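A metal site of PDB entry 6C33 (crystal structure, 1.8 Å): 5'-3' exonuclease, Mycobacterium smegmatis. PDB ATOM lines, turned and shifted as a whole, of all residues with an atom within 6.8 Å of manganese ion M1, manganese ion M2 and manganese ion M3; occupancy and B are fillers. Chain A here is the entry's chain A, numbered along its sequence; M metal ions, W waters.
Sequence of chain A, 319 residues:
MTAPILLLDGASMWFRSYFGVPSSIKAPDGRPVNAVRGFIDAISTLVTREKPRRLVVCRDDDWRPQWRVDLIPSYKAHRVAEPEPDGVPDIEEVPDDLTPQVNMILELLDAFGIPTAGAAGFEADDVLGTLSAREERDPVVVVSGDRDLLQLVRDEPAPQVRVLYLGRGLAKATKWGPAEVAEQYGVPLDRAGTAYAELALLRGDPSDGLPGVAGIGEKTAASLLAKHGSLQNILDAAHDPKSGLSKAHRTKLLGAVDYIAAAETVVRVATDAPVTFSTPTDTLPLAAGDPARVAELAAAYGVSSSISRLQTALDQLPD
Of the 23 residues printed, 2 come within 4 Å of manganese ion M2.
The nearest printed residue that does not touch manganese ion M2 is Asp 60 (4.1 Å).
Within 4 Å of manganese ion M3: Asp 148, Asp 205 and Asp 208.
The nearest printed residue that does not touch manganese ion M3 is Asp 146 (4.5 Å).
Four residues have an atom within 4 Å of manganese ion M1: Asp 125, Asp 146, Asp 148 and Asp 208.
Along chain A the residues within 4 Å of manganese ion M1 span positions 125 to 208.
The nearest printed residue that does not touch manganese ion M1 is Glu 123 (4.2 Å).
The backbone NH (N) of Asp 146 sits at hydrogen-bond distance from the side-chain hydroxyl (OG) of Ser 144, 3.0 Å away.
O of Asp 208 lies within hydrogen-bond range of N of Lys 76, at 2.7 Å.
The side-chain carboxylate (OD1) of Asp 205 lies within hydrogen-bond range of the side-chain hydroxyl (OG) of Ser 207.
O of Leu 210 is in hydrogen-bond range of N of Asp 205, at 2.8 Å.
Water W3 bridges OH of Tyr 75 (2.9 Å) and OE1 of Glu 123 (2.9 Å).
Water W5 bridges the side-chain carboxylate (OD1) of Asp 9 (2.7 Å) and the side-chain carboxylate (OD1) of Asp 60 (2.8 Å).
Water W6 lies within hydrogen-bond range of OD2 of Asp 60 (2.6 Å), OE1 of Glu 123 (2.9 Å) and NZ of Lys 76 (3.4 Å).
Manganese ion M3 is bound by water W2 (1.9 Å), OD2 of Asp 208 (2.1 Å), OD1 of Asp 148 (2.2 Å), OD2 of Asp 205 (2.2 Å), water W7 (2.2 Å) and OD2 of Asp 148 (2.3 Å).
Manganese ion M1 is bound by water W1 (2.0 Å), OD2 of Asp 146 (2.1 Å), OD2 of Asp 148 (2.2 Å), OD2 of Asp 125 (2.2 Å), water W8 (2.3 Å) and water W3 (2.3 Å).
Manganese ion M1 has six donor atoms within binding distance.
Manganese ion M2 is bound by water W1 (2.0 Å), water W6 (2.2 Å), water W5 (2.2 Å), water W4 (2.2 Å), the side-chain carboxylate (OD1) of Asp 125 (2.3 Å) and water W9 (2.3 Å).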
ATOM      1  N   ASP A   9      23.273  -4.683  26.788  1.00  0.00           N
ATOM      2  CA  ASP A   9      23.557  -5.207  25.441  1.00  0.00           C
ATOM      3  C   ASP A   9      22.210  -5.324  24.740  1.00  0.00           C
ATOM      4  O   ASP A   9      21.519  -6.335  24.869  1.00  0.00           O
ATOM      5  CB  ASP A   9      24.281  -6.542  25.538  1.00  0.00           C
ATOM      6  CG  ASP A   9      24.697  -7.097  24.184  1.00  0.00           C
ATOM      7  OD1 ASP A   9      24.249  -6.609  23.133  1.00  0.00           O
ATOM      8  OD2 ASP A   9      25.476  -8.074  24.214  1.00  0.00           O
ATOM      9  N   ALA A  11      20.858  -5.775  21.689  1.00  0.00           N
ATOM     10  CA  ALA A  11      20.487  -6.852  20.782  1.00  0.00           C
ATOM     11  C   ALA A  11      20.506  -8.194  21.497  1.00  0.00           C
ATOM     12  O   ALA A  11      19.674  -9.066  21.208  1.00  0.00           O
ATOM     13  CB  ALA A  11      21.423  -6.860  19.579  1.00  0.00           C
ATOM     14  N   SER A  12      21.437  -8.399  22.415  1.00  0.00           N
ATOM     15  CA  SER A  12      21.375  -9.623  23.218  1.00  0.00           C
ATOM     16  C   SER A  12      20.029  -9.731  23.907  1.00  0.00           C
ATOM     17  O   SER A  12      19.385 -10.787  23.872  1.00  0.00           O
ATOM     18  CB  SER A  12      22.511  -9.651  24.252  1.00  0.00           C
ATOM     19  OG  SER A  12      22.346 -10.794  25.084  1.00  0.00           O
ATOM     20  N   ASP A  60      24.224  -1.657  18.293  1.00  0.00           N
ATOM     21  CA  ASP A  60      25.109  -2.171  17.249  1.00  0.00           C
ATOM     22  C   ASP A  60      24.992  -1.242  16.037  1.00  0.00           C
ATOM     23  O   ASP A  60      24.207  -1.476  15.129  1.00  0.00           O
ATOM     24  CB  ASP A  60      24.711  -3.591  16.869  1.00  0.00           C
ATOM     25  CG  ASP A  60      25.144  -4.619  17.880  1.00  0.00           C
ATOM     26  OD1 ASP A  60      24.295  -5.053  18.713  1.00  0.00           O
ATOM     27  OD2 ASP A  60      26.333  -4.970  17.845  1.00  0.00           O
ATOM     28  N   TRP A  63      26.778  -4.319  13.448  1.00  0.00           N
ATOM     29  CA  TRP A  63      26.823  -5.616  14.121  1.00  0.00           C
ATOM     30  C   TRP A  63      27.967  -6.502  13.626  1.00  0.00           C
ATOM     31  O   TRP A  63      28.338  -7.439  14.337  1.00  0.00           O
ATOM     32  CB  TRP A  63      25.504  -6.356  13.938  1.00  0.00           C
ATOM     33  CG  TRP A  63      25.327  -6.861  12.548  1.00  0.00           C
ATOM     34  CD1 TRP A  63      24.976  -6.140  11.447  1.00  0.00           C
ATOM     35  CD2 TRP A  63      25.519  -8.211  12.097  1.00  0.00           C
ATOM     36  NE1 TRP A  63      24.923  -6.961  10.336  1.00  0.00           N
ATOM     37  CE2 TRP A  63      25.254  -8.232  10.710  1.00  0.00           C
ATOM     38  CE3 TRP A  63      25.891  -9.409  12.736  1.00  0.00           C
ATOM     39  CZ2 TRP A  63      25.356  -9.398   9.947  1.00  0.00           C
ATOM     40  CZ3 TRP A  63      25.988 -10.559  11.977  1.00  0.00           C
ATOM     41  CH2 TRP A  63      25.711 -10.548  10.597  1.00  0.00           C
ATOM     42  N   TYR A  75      34.321 -14.432  10.339  1.00  0.00           N
ATOM     43  CA  TYR A  75      33.691 -13.789  11.484  1.00  0.00           C
ATOM     44  C   TYR A  75      32.239 -13.460  11.190  1.00  0.00           C
ATOM     45  O   TYR A  75      31.949 -12.633  10.326  1.00  0.00           O
ATOM     46  CB  TYR A  75      34.463 -12.520  11.842  1.00  0.00           C
ATOM     47  CG  TYR A  75      33.916 -11.803  13.047  1.00  0.00           C
ATOM     48  CD1 TYR A  75      34.019 -12.360  14.292  1.00  0.00           C
ATOM     49  CD2 TYR A  75      33.289 -10.555  12.913  1.00  0.00           C
ATOM     50  CE1 TYR A  75      33.527 -11.705  15.419  1.00  0.00           C
ATOM     51  CE2 TYR A  75      32.791  -9.891  14.020  1.00  0.00           C
ATOM     52  CZ  TYR A  75      32.924 -10.469  15.268  1.00  0.00           C
ATOM     53  OH  TYR A  75      32.459  -9.820  16.384  1.00  0.00           O
ATOM     54  N   LYS A  76      31.333 -14.105  11.940  1.00  0.00           N
ATOM     55  CA  LYS A  76      29.883 -13.945  11.832  1.00  0.00           C
ATOM     56  C   LYS A  76      29.349 -14.208  10.429  1.00  0.00           C
ATOM     57  O   LYS A  76      28.220 -13.829  10.121  1.00  0.00           O
ATOM     58  CB  LYS A  76      29.431 -12.557  12.298  1.00  0.00           C
ATOM     59  CG  LYS A  76      29.715 -12.310  13.775  1.00  0.00           C
ATOM     60  CD  LYS A  76      29.101 -11.001  14.263  1.00  0.00           C
ATOM     61  CE  LYS A  76      29.335 -10.830  15.766  1.00  0.00           C
ATOM     62  NZ  LYS A  76      28.458  -9.767  16.339  1.00  0.00           N
ATOM     63  N   ARG A  79      25.906 -15.813   9.868  1.00  0.00           N
ATOM     64  CA  ARG A  79      24.741 -15.044  10.291  1.00  0.00           C
ATOM     65  C   ARG A  79      24.368 -13.936   9.333  1.00  0.00           C
ATOM     66  O   ARG A  79      23.456 -13.151   9.636  1.00  0.00           O
ATOM     67  CB  ARG A  79      24.986 -14.446  11.688  1.00  0.00           C
ATOM     68  CG  ARG A  79      25.234 -15.505  12.749  1.00  0.00           C
ATOM     69  CD  ARG A  79      25.002 -14.950  14.126  1.00  0.00           C
ATOM     70  NE  ARG A  79      26.230 -14.799  14.866  1.00  0.00           N
ATOM     71  CZ  ARG A  79      26.431 -13.872  15.790  1.00  0.00           C
ATOM     72  NH1 ARG A  79      25.470 -12.996  16.082  1.00  0.00           N
ATOM     73  NH2 ARG A  79      27.589 -13.806  16.426  1.00  0.00           N
ATOM     74  N   GLU A 123      30.572  -2.631  17.176  1.00  0.00           N
ATOM     75  CA  GLU A 123      29.532  -3.453  17.768  1.00  0.00           C
ATOM     76  C   GLU A 123      29.129  -2.894  19.125  1.00  0.00           C
ATOM     77  O   GLU A 123      29.855  -2.134  19.774  1.00  0.00           O
ATOM     78  CB  GLU A 123      30.019  -4.873  17.951  1.00  0.00           C
ATOM     79  CG  GLU A 123      30.341  -5.559  16.656  1.00  0.00           C
ATOM     80  CD  GLU A 123      30.735  -7.002  16.840  1.00  0.00           C
ATOM     81  OE1 GLU A 123      30.061  -7.722  17.612  1.00  0.00           O
ATOM     82  OE2 GLU A 123      31.716  -7.427  16.193  1.00  0.00           O
ATOM     83  N   ALA A 124      27.940  -3.311  19.577  1.00  0.00           N
ATOM     84  CA  ALA A 124      27.557  -2.967  20.943  1.00  0.00           C
ATOM     85  C   ALA A 124      28.565  -3.532  21.927  1.00  0.00           C
ATOM     86  O   ALA A 124      28.831  -2.919  22.971  1.00  0.00           O
ATOM     87  CB  ALA A 124      26.146  -3.475  21.239  1.00  0.00           C
ATOM     88  N   ASP A 125      29.184  -4.677  21.582  1.00  0.00           N
ATOM     89  CA  ASP A 125      30.238  -5.228  22.422  1.00  0.00           C
ATOM     90  C   ASP A 125      31.343  -4.208  22.680  1.00  0.00           C
ATOM     91  O   ASP A 125      31.861  -4.104  23.794  1.00  0.00           O
ATOM     92  CB  ASP A 125      30.840  -6.474  21.780  1.00  0.00           C
ATOM     93  CG  ASP A 125      29.808  -7.516  21.410  1.00  0.00           C
ATOM     94  OD1 ASP A 125      28.662  -7.154  21.039  1.00  0.00           O
ATOM     95  OD2 ASP A 125      30.159  -8.715  21.483  1.00  0.00           O
ATOM     96  N   LEU A 128      30.054  -1.304  24.898  1.00  0.00           N
ATOM     97  CA  LEU A 128      30.075  -1.779  26.279  1.00  0.00           C
ATOM     98  C   LEU A 128      31.488  -1.763  26.840  1.00  0.00           C
ATOM     99  O   LEU A 128      31.718  -1.288  27.959  1.00  0.00           O
ATOM    100  CB  LEU A 128      29.466  -3.186  26.340  1.00  0.00           C
ATOM    101  CG  LEU A 128      27.960  -3.214  26.083  1.00  0.00           C
ATOM    102  CD1 LEU A 128      27.470  -4.613  25.679  1.00  0.00           C
ATOM    103  CD2 LEU A 128      27.214  -2.757  27.321  1.00  0.00           C
ATOM    104  N   SER A 144      24.025  -8.858  29.628  1.00  0.00           N
ATOM    105  CA  SER A 144      24.134  -9.480  28.311  1.00  0.00           C
ATOM    106  C   SER A 144      24.117 -11.002  28.440  1.00  0.00           C
ATOM    107  O   SER A 144      24.585 -11.552  29.433  1.00  0.00           O
ATOM    108  CB  SER A 144      25.431  -9.063  27.601  1.00  0.00           C
ATOM    109  OG  SER A 144      25.513  -9.673  26.318  1.00  0.00           O
ATOM    110  N   ASP A 146      25.758 -12.612  26.017  1.00  0.00           N
ATOM    111  CA  ASP A 146      26.902 -12.905  25.150  1.00  0.00           C
ATOM    112  C   ASP A 146      28.137 -13.092  26.020  1.00  0.00           C
ATOM    113  O   ASP A 146      28.581 -12.151  26.684  1.00  0.00           O
ATOM    114  CB  ASP A 146      27.087 -11.758  24.167  1.00  0.00           C
ATOM    115  CG  ASP A 146      28.246 -11.944  23.222  1.00  0.00           C
ATOM    116  OD1 ASP A 146      28.958 -12.971  23.278  1.00  0.00           O
ATOM    117  OD2 ASP A 146      28.459 -11.023  22.388  1.00  0.00           O
ATOM    118  N   ARG A 147      28.695 -14.308  26.016  1.00  0.00           N
ATOM    119  CA  ARG A 147      29.881 -14.548  26.846  1.00  0.00           C
ATOM    120  C   ARG A 147      31.089 -13.730  26.411  1.00  0.00           C
ATOM    121  O   ARG A 147      32.036 -13.603  27.205  1.00  0.00           O
ATOM    122  CB  ARG A 147      30.233 -16.043  26.836  1.00  0.00           C
ATOM    123  CG  ARG A 147      29.354 -16.864  27.732  1.00  0.00           C
ATOM    124  CD  ARG A 147      29.711 -18.330  27.633  1.00  0.00           C
ATOM    125  NE  ARG A 147      29.710 -18.803  26.257  1.00  0.00           N
ATOM    126  CZ  ARG A 147      29.519 -20.074  25.900  1.00  0.00           C
ATOM    127  NH1 ARG A 147      29.316 -20.999  26.820  1.00  0.00           N
ATOM    128  NH2 ARG A 147      29.533 -20.407  24.624  1.00  0.00           N
ATOM    129  N   ASP A 148      31.084 -13.153  25.208  1.00  0.00           N
ATOM    130  CA  ASP A 148      32.152 -12.224  24.828  1.00  0.00           C
ATOM    131  C   ASP A 148      32.393 -11.178  25.900  1.00  0.00           C
ATOM    132  O   ASP A 148      33.530 -10.730  26.090  1.00  0.00           O
ATOM    133  CB  ASP A 148      31.819 -11.483  23.533  1.00  0.00           C
ATOM    134  CG  ASP A 148      31.816 -12.371  22.307  1.00  0.00           C
ATOM    135  OD1 ASP A 148      32.383 -13.489  22.354  1.00  0.00           O
ATOM    136  OD2 ASP A 148      31.229 -11.939  21.270  1.00  0.00           O
ATOM    137  N   LEU A 149      31.343 -10.758  26.595  1.00  0.00           N
ATOM    138  CA  LEU A 149      31.509  -9.649  27.519  1.00  0.00           C
ATOM    139  C   LEU A 149      32.130 -10.072  28.839  1.00  0.00           C
ATOM    140  O   LEU A 149      32.470  -9.197  29.640  1.00  0.00           O
ATOM    141  CB  LEU A 149      30.185  -8.943  27.737  1.00  0.00           C
ATOM    142  CG  LEU A 149      29.820  -8.353  26.363  1.00  0.00           C
ATOM    143  CD1 LEU A 149      28.411  -7.964  26.316  1.00  0.00           C
ATOM    144  CD2 LEU A 149      30.710  -7.152  26.014  1.00  0.00           C
ATOM    145  N   ASP A 205      35.227 -19.878  18.807  1.00  0.00           N
ATOM    146  CA  ASP A 205      33.971 -19.203  19.133  1.00  0.00           C
ATOM    147  C   ASP A 205      32.997 -19.522  18.012  1.00  0.00           C
ATOM    148  O   ASP A 205      32.893 -18.780  17.027  1.00  0.00           O
ATOM    149  CB  ASP A 205      34.187 -17.702  19.277  1.00  0.00           C
ATOM    150  CG  ASP A 205      32.953 -16.955  19.761  1.00  0.00           C
ATOM    151  OD1 ASP A 205      31.833 -17.504  19.759  1.00  0.00           O
ATOM    152  OD2 ASP A 205      33.127 -15.781  20.129  1.00  0.00           O
ATOM    153  N   SER A 207      29.693 -19.508  17.696  1.00  0.00           N
ATOM    154  CA  SER A 207      28.602 -18.586  17.396  1.00  0.00           C
ATOM    155  C   SER A 207      29.071 -17.383  16.581  1.00  0.00           C
ATOM    156  O   SER A 207      28.292 -16.830  15.800  1.00  0.00           O
ATOM    157  CB  SER A 207      27.910 -18.127  18.690  1.00  0.00           C
ATOM    158  OG  SER A 207      28.852 -17.814  19.701  1.00  0.00           O
ATOM    159  N   ASP A 208      30.336 -16.971  16.728  1.00  0.00           N
ATOM    160  CA  ASP A 208      30.871 -15.885  15.922  1.00  0.00           C
ATOM    161  C   ASP A 208      31.664 -16.368  14.710  1.00  0.00           C
ATOM    162  O   ASP A 208      32.272 -15.561  14.002  1.00  0.00           O
ATOM    163  CB  ASP A 208      31.747 -14.974  16.789  1.00  0.00           C
ATOM    164  CG  ASP A 208      30.947 -13.895  17.525  1.00  0.00           C
ATOM    165  OD1 ASP A 208      29.712 -13.790  17.326  1.00  0.00           O
ATOM    166  OD2 ASP A 208      31.573 -13.150  18.292  1.00  0.00           O
ATOM    167  N   LEU A 210      34.462 -18.175  14.583  1.00  0.00           N
ATOM    168  CA  LEU A 210      35.917 -18.141  14.760  1.00  0.00           C
ATOM    169  C   LEU A 210      36.417 -19.537  15.077  1.00  0.00           C
ATOM    170  O   LEU A 210      36.023 -20.093  16.110  1.00  0.00           O
ATOM    171  CB  LEU A 210      36.289 -17.176  15.875  1.00  0.00           C
ATOM    172  CG  LEU A 210      35.889 -15.738  15.595  1.00  0.00           C
ATOM    173  CD1 LEU A 210      36.096 -14.868  16.821  1.00  0.00           C
ATOM    174  CD2 LEU A 210      36.678 -15.205  14.378  1.00  0.00           C
ATOM    175  N   VAL A 267      38.833 -10.638  18.575  1.00  0.00           N
ATOM    176  CA  VAL A 267      38.186 -11.196  19.775  1.00  0.00           C
ATOM    177  C   VAL A 267      38.078 -10.158  20.883  1.00  0.00           C
ATOM    178  O   VAL A 267      37.079 -10.128  21.626  1.00  0.00           O
ATOM    179  CB  VAL A 267      38.970 -12.449  20.237  1.00  0.00           C
ATOM    180  CG1 VAL A 267      38.495 -12.912  21.603  1.00  0.00           C
ATOM    181  CG2 VAL A 267      38.822 -13.568  19.222  1.00  0.00           C
ATOM    182  N   VAL A 269      37.238  -6.798  22.635  1.00  0.00           N
ATOM    183  CA  VAL A 269      36.351  -5.663  22.403  1.00  0.00           C
ATOM    184  C   VAL A 269      37.180  -4.381  22.447  1.00  0.00           C
ATOM    185  O   VAL A 269      38.141  -4.265  23.227  1.00  0.00           O
ATOM    186  CB  VAL A 269      35.198  -5.624  23.423  1.00  0.00           C
ATOM    187  CG1 VAL A 269      34.464  -6.951  23.423  1.00  0.00           C
ATOM    188  CG2 VAL A 269      35.726  -5.309  24.810  1.00  0.00           C
HETATM  189 MN    MN M   1      29.597 -10.641  20.630  1.00  0.00          MN
HETATM  190 MN    MN M   2      26.884  -8.272  20.170  1.00  0.00          MN
HETATM  191 MN    MN M   3      32.195 -13.806  20.230  1.00  0.00          MN
HETATM  192  O   HOH W   1      28.000  -9.841  19.656  1.00  0.00           O
HETATM  193  O   HOH W   2      30.683 -14.918  20.701  1.00  0.00           O
HETATM  194  O   HOH W   3      30.915 -10.271  18.805  1.00  0.00           O
HETATM  195  O   HOH W   4      26.467  -9.242  22.093  1.00  0.00           O
HETATM  196  O   HOH W   5      25.423  -6.755  20.668  1.00  0.00           O
HETATM  197  O   HOH W   6      27.311  -7.298  18.297  1.00  0.00           O
HETATM  198  O   HOH W   7      33.997 -12.617  19.843  1.00  0.00           O
HETATM  199  O   HOH W   8      28.697 -12.481  19.644  1.00  0.00           O
HETATM  200  O   HOH W   9      25.200  -9.439  19.172  1.00  0.00           O
